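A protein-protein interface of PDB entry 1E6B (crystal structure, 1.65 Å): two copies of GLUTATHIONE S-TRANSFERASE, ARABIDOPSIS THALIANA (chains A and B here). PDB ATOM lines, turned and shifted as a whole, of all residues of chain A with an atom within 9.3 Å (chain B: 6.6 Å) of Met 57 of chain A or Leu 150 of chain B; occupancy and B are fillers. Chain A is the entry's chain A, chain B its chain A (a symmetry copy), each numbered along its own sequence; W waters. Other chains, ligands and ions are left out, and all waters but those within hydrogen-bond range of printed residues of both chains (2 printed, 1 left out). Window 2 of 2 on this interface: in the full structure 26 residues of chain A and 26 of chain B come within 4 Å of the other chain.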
ATOM      1  N   GLN A  46      14.738 -14.563  10.249  1.00  0.00           N
ATOM      2  CA  GLN A  46      13.323 -14.231  10.334  1.00  0.00           C
ATOM      3  C   GLN A  46      12.418 -15.213   9.587  1.00  0.00           C
ATOM      4  O   GLN A  46      11.194 -15.118   9.619  1.00  0.00           O
ATOM      5  CB  GLN A  46      13.051 -12.805   9.865  1.00  0.00           C
ATOM      6  CG  GLN A  46      13.223 -12.508   8.398  1.00  0.00           C
ATOM      7  CD  GLN A  46      14.610 -12.296   7.873  1.00  0.00           C
ATOM      8  OE1 GLN A  46      15.628 -12.876   8.277  1.00  0.00           O
ATOM      9  NE2 GLN A  46      14.726 -11.338   6.937  1.00  0.00           N
ATOM     10  N   PHE A  47      12.998 -16.132   8.803  1.00  0.00           N
ATOM     11  CA  PHE A  47      12.207 -17.135   8.085  1.00  0.00           C
ATOM     12  C   PHE A  47      12.279 -18.500   8.764  1.00  0.00           C
ATOM     13  O   PHE A  47      11.760 -19.481   8.236  1.00  0.00           O
ATOM     14  CB  PHE A  47      12.657 -17.226   6.625  1.00  0.00           C
ATOM     15  CG  PHE A  47      12.565 -15.890   5.946  1.00  0.00           C
ATOM     16  CD1 PHE A  47      11.316 -15.316   5.713  1.00  0.00           C
ATOM     17  CD2 PHE A  47      13.685 -15.198   5.567  1.00  0.00           C
ATOM     18  CE1 PHE A  47      11.197 -14.104   5.057  1.00  0.00           C
ATOM     19  CE2 PHE A  47      13.593 -13.969   4.931  1.00  0.00           C
ATOM     20  CZ  PHE A  47      12.340 -13.419   4.700  1.00  0.00           C
ATOM     21  N   PHE A  51      10.620 -19.269  15.138  1.00  0.00           N
ATOM     22  CA  PHE A  51      10.411 -17.826  15.303  1.00  0.00           C
ATOM     23  C   PHE A  51       9.044 -17.436  14.752  1.00  0.00           C
ATOM     24  O   PHE A  51       8.290 -16.672  15.347  1.00  0.00           O
ATOM     25  CB  PHE A  51      11.536 -17.132  14.552  1.00  0.00           C
ATOM     26  CG  PHE A  51      11.343 -15.671  14.293  1.00  0.00           C
ATOM     27  CD1 PHE A  51      11.544 -14.746  15.303  1.00  0.00           C
ATOM     28  CD2 PHE A  51      10.930 -15.209  13.056  1.00  0.00           C
ATOM     29  CE1 PHE A  51      11.372 -13.397  15.068  1.00  0.00           C
ATOM     30  CE2 PHE A  51      10.750 -13.864  12.805  1.00  0.00           C
ATOM     31  CZ  PHE A  51      10.991 -12.950  13.830  1.00  0.00           C
ATOM     32  N   LYS A  52       8.667 -18.030  13.620  1.00  0.00           N
ATOM     33  CA  LYS A  52       7.383 -17.889  12.959  1.00  0.00           C
ATOM     34  C   LYS A  52       6.232 -18.356  13.832  1.00  0.00           C
ATOM     35  O   LYS A  52       5.135 -17.821  13.802  1.00  0.00           O
ATOM     36  CB  LYS A  52       7.400 -18.707  11.660  1.00  0.00           C
ATOM     37  CG  LYS A  52       8.003 -17.948  10.482  1.00  0.00           C
ATOM     38  CD  LYS A  52       6.844 -17.208   9.799  1.00  0.00           C
ATOM     39  CE  LYS A  52       7.050 -17.296   8.296  1.00  0.00           C
ATOM     40  NZ  LYS A  52       5.758 -17.461   7.575  1.00  0.00           N
ATOM     41  N   LYS A  53       6.507 -19.331  14.696  1.00  0.00           N
ATOM     42  CA  LYS A  53       5.528 -19.803  15.654  1.00  0.00           C
ATOM     43  C   LYS A  53       5.202 -18.730  16.689  1.00  0.00           C
ATOM     44  O   LYS A  53       4.068 -18.587  17.126  1.00  0.00           O
ATOM     45  CB  LYS A  53       6.071 -21.048  16.385  1.00  0.00           C
ATOM     46  CG  LYS A  53       4.944 -21.763  17.109  1.00  0.00           C
ATOM     47  CD  LYS A  53       4.966 -21.515  18.616  1.00  0.00           C
ATOM     48  CE  LYS A  53       3.702 -22.092  19.256  1.00  0.00           C
ATOM     49  NZ  LYS A  53       4.049 -22.942  20.439  1.00  0.00           N
ATOM     50  N   ILE A  54       6.248 -18.049  17.152  1.00  0.00           N
ATOM     51  CA  ILE A  54       6.083 -17.008  18.151  1.00  0.00           C
ATOM     52  C   ILE A  54       5.625 -15.699  17.511  1.00  0.00           C
ATOM     53  O   ILE A  54       4.808 -14.997  18.085  1.00  0.00           O
ATOM     54  CB  ILE A  54       7.385 -16.722  18.928  1.00  0.00           C
ATOM     55  CG1 ILE A  54       7.739 -18.000  19.695  1.00  0.00           C
ATOM     56  CG2 ILE A  54       7.228 -15.515  19.849  1.00  0.00           C
ATOM     57  CD1 ILE A  54       8.599 -17.855  20.920  1.00  0.00           C
ATOM     58  N   ASN A  55       6.106 -15.405  16.341  1.00  0.00           N
ATOM     59  CA  ASN A  55       5.847 -14.195  15.564  1.00  0.00           C
ATOM     60  C   ASN A  55       5.323 -14.521  14.186  1.00  0.00           C
ATOM     61  O   ASN A  55       5.991 -14.425  13.151  1.00  0.00           O
ATOM     62  CB  ASN A  55       7.236 -13.510  15.485  1.00  0.00           C
ATOM     63  CG  ASN A  55       7.182 -12.141  14.835  1.00  0.00           C
ATOM     64  OD1 ASN A  55       6.111 -11.563  14.783  1.00  0.00           O
ATOM     65  ND2 ASN A  55       8.304 -11.655  14.322  1.00  0.00           N
ATOM     66  N   PRO A  56       4.068 -14.966  14.105  1.00  0.00           N
ATOM     67  CA  PRO A  56       3.428 -15.379  12.869  1.00  0.00           C
ATOM     68  C   PRO A  56       3.468 -14.323  11.800  1.00  0.00           C
ATOM     69  O   PRO A  56       3.628 -14.631  10.630  1.00  0.00           O
ATOM     70  CB  PRO A  56       2.004 -15.766  13.230  1.00  0.00           C
ATOM     71  CG  PRO A  56       1.807 -15.398  14.640  1.00  0.00           C
ATOM     72  CD  PRO A  56       3.140 -15.089  15.246  1.00  0.00           C
ATOM     73  N   MET A  57       3.398 -13.022  12.190  1.00  0.00           N
ATOM     74  CA  MET A  57       3.530 -11.993  11.188  1.00  0.00           C
ATOM     75  C   MET A  57       4.932 -12.050  10.587  1.00  0.00           C
ATOM     76  O   MET A  57       5.098 -11.566   9.469  1.00  0.00           O
ATOM     77  CB  MET A  57       3.186 -10.595  11.674  1.00  0.00           C
ATOM     78  CG  MET A  57       1.751 -10.390  12.116  1.00  0.00           C
ATOM     79  SD  MET A  57       0.514 -10.689  10.844  1.00  0.00           S
ATOM     80  CE  MET A  57       0.885  -9.361   9.711  1.00  0.00           C
ATOM     81  N   GLY A  58       5.943 -12.559  11.329  1.00  0.00           N
ATOM     82  CA  GLY A  58       7.258 -12.725  10.767  1.00  0.00           C
ATOM     83  C   GLY A  58       8.162 -11.540  10.626  1.00  0.00           C
ATOM     84  O   GLY A  58       9.255 -11.628  10.045  1.00  0.00           O
ATOM     85  N   THR A  59       7.721 -10.371  11.114  1.00  0.00           N
ATOM     86  CA  THR A  59       8.546  -9.180  10.899  1.00  0.00           C
ATOM     87  C   THR A  59       9.304  -8.797  12.166  1.00  0.00           C
ATOM     88  O   THR A  59       8.929  -9.141  13.286  1.00  0.00           O
ATOM     89  CB  THR A  59       7.654  -8.018  10.440  1.00  0.00           C
ATOM     90  OG1 THR A  59       6.553  -7.874  11.355  1.00  0.00           O
ATOM     91  CG2 THR A  59       7.068  -8.336   9.049  1.00  0.00           C
ATOM     92  N   VAL A  60      10.352  -8.026  11.936  1.00  0.00           N
ATOM     93  CA  VAL A  60      11.205  -7.454  13.015  1.00  0.00           C
ATOM     94  C   VAL A  60      11.240  -5.950  12.817  1.00  0.00           C
ATOM     95  O   VAL A  60      11.429  -5.472  11.676  1.00  0.00           O
ATOM     96  CB  VAL A  60      12.617  -8.056  12.807  1.00  0.00           C
ATOM     97  CG1 VAL A  60      13.651  -7.321  13.641  1.00  0.00           C
ATOM     98  CG2 VAL A  60      12.559  -9.544  13.143  1.00  0.00           C
ATOM     99  N   PRO A  61      11.011  -5.119  13.840  1.00  0.00           N
ATOM    100  CA  PRO A  61      10.873  -5.536  15.198  1.00  0.00           C
ATOM    101  C   PRO A  61       9.551  -6.145  15.577  1.00  0.00           C
ATOM    102  O   PRO A  61       8.532  -5.979  14.885  1.00  0.00           O
ATOM    103  CB  PRO A  61      11.077  -4.219  16.023  1.00  0.00           C
ATOM    104  CG  PRO A  61      10.479  -3.185  15.082  1.00  0.00           C
ATOM    105  CD  PRO A  61      11.061  -3.629  13.735  1.00  0.00           C
ATOM    106  N   ALA A  62       9.566  -6.924  16.666  1.00  0.00           N
ATOM    107  CA  ALA A  62       8.353  -7.532  17.188  1.00  0.00           C
ATOM    108  C   ALA A  62       8.445  -7.462  18.715  1.00  0.00           C
ATOM    109  O   ALA A  62       9.473  -7.853  19.260  1.00  0.00           O
ATOM    110  CB  ALA A  62       8.054  -8.941  16.671  1.00  0.00           C
ATOM    111  N   VAL A  69       1.678 -10.159  20.896  1.00  0.00           N
ATOM    112  CA  VAL A  69       2.769  -9.921  19.986  1.00  0.00           C
ATOM    113  C   VAL A  69       2.377  -8.742  19.094  1.00  0.00           C
ATOM    114  O   VAL A  69       1.334  -8.822  18.430  1.00  0.00           O
ATOM    115  CB  VAL A  69       3.135 -11.107  19.088  1.00  0.00           C
ATOM    116  CG1 VAL A  69       4.247 -10.725  18.122  1.00  0.00           C
ATOM    117  CG2 VAL A  69       3.581 -12.290  19.946  1.00  0.00           C
ATOM    118  N   ILE A  70       3.187  -7.709  19.118  1.00  0.00           N
ATOM    119  CA  ILE A  70       2.912  -6.526  18.310  1.00  0.00           C
ATOM    120  C   ILE A  70       4.024  -6.385  17.280  1.00  0.00           C
ATOM    121  O   ILE A  70       5.213  -6.306  17.669  1.00  0.00           O
ATOM    122  CB  ILE A  70       2.864  -5.218  19.123  1.00  0.00           C
ATOM    123  CG1 ILE A  70       2.081  -5.278  20.428  1.00  0.00           C
ATOM    124  CG2 ILE A  70       2.390  -4.064  18.246  1.00  0.00           C
ATOM    125  CD1 ILE A  70       0.601  -5.470  20.377  1.00  0.00           C
ATOM    126  N   ASN A  71       3.666  -6.225  16.016  1.00  0.00           N
ATOM    127  CA  ASN A  71       4.609  -5.954  14.963  1.00  0.00           C
ATOM    128  C   ASN A  71       4.360  -4.512  14.492  1.00  0.00           C
ATOM    129  O   ASN A  71       3.355  -3.910  14.915  1.00  0.00           O
ATOM    130  CB  ASN A  71       4.440  -6.871  13.738  1.00  0.00           C
ATOM    131  CG  ASN A  71       4.550  -8.329  14.189  1.00  0.00           C
ATOM    132  OD1 ASN A  71       3.639  -8.979  14.699  1.00  0.00           O
ATOM    133  ND2 ASN A  71       5.729  -8.843  14.013  1.00  0.00           N
ATOM    134  N   ASP A  72       5.281  -4.049  13.659  1.00  0.00           N
ATOM    135  CA  ASP A  72       5.296  -2.690  13.140  1.00  0.00           C
ATOM    136  C   ASP A  72       5.847  -1.695  14.151  1.00  0.00           C
ATOM    137  O   ASP A  72       5.310  -1.502  15.235  1.00  0.00           O
ATOM    138  CB  ASP A  72       3.908  -2.235  12.609  1.00  0.00           C
ATOM    139  CG  ASP A  72       4.072  -0.856  11.992  1.00  0.00           C
ATOM    140  OD1 ASP A  72       4.615  -0.800  10.859  1.00  0.00           O
ATOM    141  OD2 ASP A  72       3.710   0.140  12.651  1.00  0.00           O
ATOM    142  N   ALA A  75       3.171   0.861  15.344  1.00  0.00           N
ATOM    143  CA  ALA A  75       2.168   0.266  16.222  1.00  0.00           C
ATOM    144  C   ALA A  75       2.845  -0.104  17.559  1.00  0.00           C
ATOM    145  O   ALA A  75       2.190   0.067  18.583  1.00  0.00           O
ATOM    146  CB  ALA A  75       1.581  -0.992  15.595  1.00  0.00           C
ATOM    147  N   ALA B  98      -3.632  -1.611  18.936  1.00  0.00           N
ATOM    148  CA  ALA B  98      -2.407  -1.954  18.219  1.00  0.00           C
ATOM    149  C   ALA B  98      -2.718  -2.636  16.877  1.00  0.00           C
ATOM    150  O   ALA B  98      -1.995  -2.380  15.915  1.00  0.00           O
ATOM    151  CB  ALA B  98      -1.528  -2.944  18.968  1.00  0.00           C
ATOM    152  N   VAL B  99      -3.690  -3.546  16.839  1.00  0.00           N
ATOM    153  CA  VAL B  99      -4.019  -4.152  15.532  1.00  0.00           C
ATOM    154  C   VAL B  99      -4.455  -3.114  14.509  1.00  0.00           C
ATOM    155  O   VAL B  99      -4.103  -3.191  13.297  1.00  0.00           O
ATOM    156  CB  VAL B  99      -5.087  -5.243  15.757  1.00  0.00           C
ATOM    157  CG1 VAL B  99      -5.528  -5.794  14.394  1.00  0.00           C
ATOM    158  CG2 VAL B  99      -4.463  -6.358  16.640  1.00  0.00           C
ATOM    159  N   ASN B 100      -5.248  -2.127  14.997  1.00  0.00           N
ATOM    160  CA  ASN B 100      -5.684  -1.083  14.054  1.00  0.00           C
ATOM    161  C   ASN B 100      -4.477  -0.331  13.503  1.00  0.00           C
ATOM    162  O   ASN B 100      -4.435  -0.078  12.305  1.00  0.00           O
ATOM    163  CB  ASN B 100      -6.591  -0.035  14.721  1.00  0.00           C
ATOM    164  CG  ASN B 100      -8.041  -0.517  14.657  1.00  0.00           C
ATOM    165  OD1 ASN B 100      -8.717  -0.251  13.648  1.00  0.00           O
ATOM    166  ND2 ASN B 100      -8.422  -1.343  15.623  1.00  0.00           N
ATOM    167  N   TYR B 101      -3.512   0.024  14.377  1.00  0.00           N
ATOM    168  CA  TYR B 101      -2.338   0.743  13.861  1.00  0.00           C
ATOM    169  C   TYR B 101      -1.502  -0.106  12.902  1.00  0.00           C
ATOM    170  O   TYR B 101      -0.913   0.433  11.932  1.00  0.00           O
ATOM    171  CB  TYR B 101      -1.469   1.176  15.032  1.00  0.00           C
ATOM    172  CG  TYR B 101      -2.037   2.220  15.975  1.00  0.00           C
ATOM    173  CD1 TYR B 101      -2.594   3.398  15.492  1.00  0.00           C
ATOM    174  CD2 TYR B 101      -1.973   1.979  17.359  1.00  0.00           C
ATOM    175  CE1 TYR B 101      -3.047   4.344  16.390  1.00  0.00           C
ATOM    176  CE2 TYR B 101      -2.443   2.939  18.247  1.00  0.00           C
ATOM    177  CZ  TYR B 101      -2.989   4.095  17.747  1.00  0.00           C
ATOM    178  OH  TYR B 101      -3.460   5.068  18.626  1.00  0.00           O
ATOM    179  N   GLN B 102      -1.448  -1.407  13.159  1.00  0.00           N
ATOM    180  CA  GLN B 102      -0.675  -2.335  12.293  1.00  0.00           C
ATOM    181  C   GLN B 102      -1.349  -2.453  10.933  1.00  0.00           C
ATOM    182  O   GLN B 102      -0.654  -2.429   9.913  1.00  0.00           O
ATOM    183  CB  GLN B 102      -0.637  -3.756  12.881  1.00  0.00           C
ATOM    184  CG  GLN B 102       0.265  -3.805  14.112  1.00  0.00           C
ATOM    185  CD  GLN B 102       0.222  -5.167  14.789  1.00  0.00           C
ATOM    186  OE1 GLN B 102       0.879  -6.080  14.273  1.00  0.00           O
ATOM    187  NE2 GLN B 102      -0.484  -5.270  15.916  1.00  0.00           N
ATOM    188  N   ALA B 103      -2.689  -2.536  10.918  1.00  0.00           N
ATOM    189  CA  ALA B 103      -3.448  -2.639   9.676  1.00  0.00           C
ATOM    190  C   ALA B 103      -3.223  -1.361   8.887  1.00  0.00           C
ATOM    191  O   ALA B 103      -2.973  -1.369   7.666  1.00  0.00           O
ATOM    192  CB  ALA B 103      -4.939  -2.853   9.970  1.00  0.00           C
ATOM    193  N   MET B 104      -3.284  -0.188   9.540  1.00  0.00           N
ATOM    194  CA  MET B 104      -3.040   1.101   8.951  1.00  0.00           C
ATOM    195  C   MET B 104      -1.640   1.119   8.294  1.00  0.00           C
ATOM    196  O   MET B 104      -1.522   1.431   7.094  1.00  0.00           O
ATOM    197  CB  MET B 104      -3.203   2.227   9.983  1.00  0.00           C
ATOM    198  CG  MET B 104      -2.961   3.634   9.417  1.00  0.00           C
ATOM    199  SD  MET B 104      -1.242   4.046   9.154  1.00  0.00           S
ATOM    200  CE  MET B 104      -0.551   4.100  10.807  1.00  0.00           C
ATOM    201  N   ILE B 106       0.336  -1.417   7.338  1.00  0.00           N
ATOM    202  CA  ILE B 106       0.527  -2.298   6.159  1.00  0.00           C
ATOM    203  C   ILE B 106      -0.005  -1.591   4.902  1.00  0.00           C
ATOM    204  O   ILE B 106       0.622  -1.565   3.825  1.00  0.00           O
ATOM    205  CB  ILE B 106      -0.156  -3.647   6.342  1.00  0.00           C
ATOM    206  CG1 ILE B 106       0.614  -4.447   7.406  1.00  0.00           C
ATOM    207  CG2 ILE B 106      -0.261  -4.405   5.010  1.00  0.00           C
ATOM    208  CD1 ILE B 106      -0.228  -5.597   7.917  1.00  0.00           C
ATOM    209  N   THR B 145      -2.279 -10.592   1.982  1.00  0.00           N
ATOM    210  CA  THR B 145      -2.019 -11.808   2.734  1.00  0.00           C
ATOM    211  C   THR B 145      -1.708 -11.391   4.172  1.00  0.00           C
ATOM    212  O   THR B 145      -2.204 -12.030   5.101  1.00  0.00           O
ATOM    213  CB  THR B 145      -0.874 -12.642   2.099  1.00  0.00           C
ATOM    214  OG1 THR B 145      -1.338 -13.032   0.798  1.00  0.00           O
ATOM    215  CG2 THR B 145      -0.543 -13.906   2.914  1.00  0.00           C
ATOM    216  N   ALA B 146      -0.878 -10.357   4.350  1.00  0.00           N
ATOM    217  CA  ALA B 146      -0.530  -9.923   5.728  1.00  0.00           C
ATOM    218  C   ALA B 146      -1.768  -9.391   6.432  1.00  0.00           C
ATOM    219  O   ALA B 146      -1.976  -9.662   7.622  1.00  0.00           O
ATOM    220  CB  ALA B 146       0.560  -8.865   5.610  1.00  0.00           C
ATOM    221  N   LEU B 147      -2.547  -8.545   5.721  1.00  0.00           N
ATOM    222  CA  LEU B 147      -3.762  -8.051   6.432  1.00  0.00           C
ATOM    223  C   LEU B 147      -4.691  -9.163   6.865  1.00  0.00           C
ATOM    224  O   LEU B 147      -5.320  -9.113   7.961  1.00  0.00           O
ATOM    225  CB  LEU B 147      -4.505  -7.070   5.513  1.00  0.00           C
ATOM    226  CG  LEU B 147      -3.798  -5.727   5.343  1.00  0.00           C
ATOM    227  CD1 LEU B 147      -4.330  -4.965   4.132  1.00  0.00           C
ATOM    228  CD2 LEU B 147      -3.995  -4.854   6.621  1.00  0.00           C
ATOM    229  N   GLU B 148      -4.881 -10.180   6.030  1.00  0.00           N
ATOM    230  CA  GLU B 148      -5.719 -11.329   6.352  1.00  0.00           C
ATOM    231  C   GLU B 148      -5.169 -12.067   7.562  1.00  0.00           C
ATOM    232  O   GLU B 148      -5.899 -12.411   8.514  1.00  0.00           O
ATOM    233  CB  GLU B 148      -5.809 -12.305   5.149  1.00  0.00           C
ATOM    234  CG  GLU B 148      -6.676 -13.500   5.476  1.00  0.00           C
ATOM    235  CD  GLU B 148      -8.166 -13.187   5.448  1.00  0.00           C
ATOM    236  OE1 GLU B 148      -8.542 -12.182   4.841  1.00  0.00           O
ATOM    237  OE2 GLU B 148      -8.925 -13.973   6.023  1.00  0.00           O
ATOM    238  N   LYS B 149      -3.854 -12.316   7.588  1.00  0.00           N
ATOM    239  CA  LYS B 149      -3.167 -12.905   8.691  1.00  0.00           C
ATOM    240  C   LYS B 149      -3.430 -12.126   9.976  1.00  0.00           C
ATOM    241  O   LYS B 149      -3.727 -12.694  11.034  1.00  0.00           O
ATOM    242  CB  LYS B 149      -1.632 -12.947   8.518  1.00  0.00           C
ATOM    243  CG  LYS B 149      -1.012 -14.016   9.431  1.00  0.00           C
ATOM    244  CD  LYS B 149       0.437 -14.309   9.043  1.00  0.00           C
ATOM    245  CE  LYS B 149       0.531 -15.195   7.814  1.00  0.00           C
ATOM    246  NZ  LYS B 149       0.818 -14.457   6.558  1.00  0.00           N
ATOM    247  N   LEU B 150      -3.316 -10.798   9.888  1.00  0.00           N
ATOM    248  CA  LEU B 150      -3.498  -9.946  11.048  1.00  0.00           C
ATOM    249  C   LEU B 150      -4.922  -9.909  11.581  1.00  0.00           C
ATOM    250  O   LEU B 150      -5.163 -10.076  12.773  1.00  0.00           O
ATOM    251  CB  LEU B 150      -3.093  -8.507  10.669  1.00  0.00           C
ATOM    252  CG  LEU B 150      -3.289  -7.405  11.717  1.00  0.00           C
ATOM    253  CD1 LEU B 150      -2.184  -7.540  12.768  1.00  0.00           C
ATOM    254  CD2 LEU B 150      -3.265  -6.027  11.073  1.00  0.00           C
ATOM    255  N   LEU B 151      -5.902  -9.813  10.675  1.00  0.00           N
ATOM    256  CA  LEU B 151      -7.283  -9.588  11.117  1.00  0.00           C
ATOM    257  C   LEU B 151      -8.176 -10.791  11.328  1.00  0.00           C
ATOM    258  O   LEU B 151      -9.227 -10.679  11.987  1.00  0.00           O
ATOM    259  CB  LEU B 151      -7.900  -8.644  10.058  1.00  0.00           C
ATOM    260  CG  LEU B 151      -7.288  -7.243   9.897  1.00  0.00           C
ATOM    261  CD1 LEU B 151      -7.972  -6.443   8.801  1.00  0.00           C
ATOM    262  CD2 LEU B 151      -7.330  -6.476  11.241  1.00  0.00           C
ATOM    263  N   VAL B 152      -7.780 -11.977  10.862  1.00  0.00           N
ATOM    264  CA  VAL B 152      -8.603 -13.163  10.918  1.00  0.00           C
ATOM    265  C   VAL B 152      -8.950 -13.559  12.331  1.00  0.00           C
ATOM    266  O   VAL B 152     -10.043 -14.100  12.608  1.00  0.00           O
ATOM    267  CB  VAL B 152      -7.919 -14.324  10.123  1.00  0.00           C
ATOM    268  CG1 VAL B 152      -6.617 -14.764  10.780  1.00  0.00           C
ATOM    269  CG2 VAL B 152      -8.931 -15.470   9.982  1.00  0.00           C
ATOM    270  N   ASN B 153      -8.150 -13.179  13.323  1.00  0.00           N
ATOM    271  CA  ASN B 153      -8.464 -13.563  14.695  1.00  0.00           C
ATOM    272  C   ASN B 153      -9.201 -12.484  15.459  1.00  0.00           C
ATOM    273  O   ASN B 153      -9.367 -12.612  16.672  1.00  0.00           O
ATOM    274  CB  ASN B 153      -7.238 -14.165  15.367  1.00  0.00           C
ATOM    275  CG  ASN B 153      -6.917 -15.504  14.702  1.00  0.00           C
ATOM    276  OD1 ASN B 153      -7.798 -16.369  14.566  1.00  0.00           O
ATOM    277  ND2 ASN B 153      -5.685 -15.650  14.233  1.00  0.00           N
ATOM    278  N   CYS B 154      -9.701 -11.459  14.773  1.00  0.00           N
ATOM    279  CA  CYS B 154     -10.501 -10.426  15.409  1.00  0.00           C
ATOM    280  C   CYS B 154     -11.991 -10.695  15.155  1.00  0.00           C
ATOM    281  O   CYS B 154     -12.438 -10.499  14.007  1.00  0.00           O
ATOM    282  CB  CYS B 154     -10.187  -9.072  14.764  1.00  0.00           C
ATOM    283  SG  CYS B 154      -8.472  -8.568  15.070  1.00  0.00           S
ATOM    284  N   ALA B 159     -13.259  -4.809  10.670  1.00  0.00           N
ATOM    285  CA  ALA B 159     -11.878  -5.269  10.862  1.00  0.00           C
ATOM    286  C   ALA B 159     -11.536  -5.699  12.273  1.00  0.00           C
ATOM    287  O   ALA B 159     -10.792  -6.692  12.442  1.00  0.00           O
ATOM    288  CB  ALA B 159     -10.916  -4.160  10.433  1.00  0.00           C
HETATM  289  O   HOH W   1      -1.200 -12.912  13.377  1.00  0.00           O
HETATM  290  O   HOH W   2      -0.914  -7.375  17.520  1.00  0.00           O
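The backbone carbonyl oxygen (O) of Ala 98 of chain B sits close to the side-chain amide nitrogen (NE2) of Gln 102 of chain B.
The side-chain hydroxyl of Thr 59 of chain A lies within hydrogen-bond range of the side-chain amide nitrogen of Asn 71 of chain A (2.9 Å).
The side-chain amide oxygen (OD1) of Asn 55 of chain A lies within hydrogen-bond range of the side-chain amide nitrogen (ND2) of Asn 71 of chain A, at 2.9 Å.
The backbone NH (N) of Ala 75 of chain A is in hydrogen-bond range of the side-chain carboxylate (OD2) of Asp 72 of chain A (2.8 Å).
Met 57 of chain A touches three residues of chain B.
Leu 150 of chain B touches just one residue of chain A: Met 57.
Leu 151 of chain B touches none of the printed residues of chain A.
Of the printed residues of chain B, Ile 70 of chain A touches Ala 98 and Gln 102.
Printed residues of chain B within 4 Å of Asn 71 of chain A: Gln 102.
Ala 103 of chain B touches none of the printed residues of chain A.
The nearest printed residue of chain B that does not touch Asn 71 of chain A is Ala 98 of chain B (5.7 Å).
Of the 19 printed residues of chain A, 5 touch a printed residue of chain B.
Hydrophobic or aromatic side chains of chain A that line the printed part of chain B: Met 57, Ile 70 and Ala 75.
Printed residues of chain B that touch a printed residue of chain A: Ala 98, Tyr 101, Gln 102, Ala 146, Lys 149 and Leu 150.
Along chain B the printed residues that touch a printed residue of chain A span positions 98 to 150.
Among the printed residues, no Asp or Glu carboxylate lies within 4 Å of a Lys or Arg side-chain nitrogen of the other chain.
No position is printed for both chains.
Of the 10 pairs that touch across the chains among the printed residues, none has its exchanged pair printed and touching as well.
Water W2 bridges the side-chain amide nitrogen (NE2) of Gln 102 of chain B (2.7 Å) and the backbone carbonyl oxygen (O) of Val 69 of chain A (2.8 Å).
Water W1 lies within hydrogen-bond range of O of Lys 149 of chain B (3.5 Å) and SD of Met 57 of chain A (3.8 Å).
The backbone NH (N) of Asn 71 of chain A sits at hydrogen-bond distance from the side-chain amide oxygen (OE1) of Gln 102 of chain B (3.3 Å).
O of Pro 56 of chain A touches CD of Lys 149 of chain B, 3.6 Å away.
Ala 146 of chain B touches Met 57 of chain A (O to CE, 3.6 Å).
Lys 149 of chain B touches Met 57 of chain A.
Leu 150 of chain B touches Met 57 of chain A (N to SD, 3.9 Å).
CB of Ala 98 of chain B touches CD1 of Ile 70 of chain A, 3.6 Å away.
Gln 102 of chain B touches Ile 70 of chain A (NE2 to CG2, 3.9 Å).
CB of Ala 75 of chain A touches O of Ala 98 of chain B (3.8 Å).
CB of Ala 75 of chain A touches CB of Tyr 101 of chain B, at 3.8 Å.
CB of Ala 75 of chain A touches CG of Gln 102 of chain B (3.4 Å).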
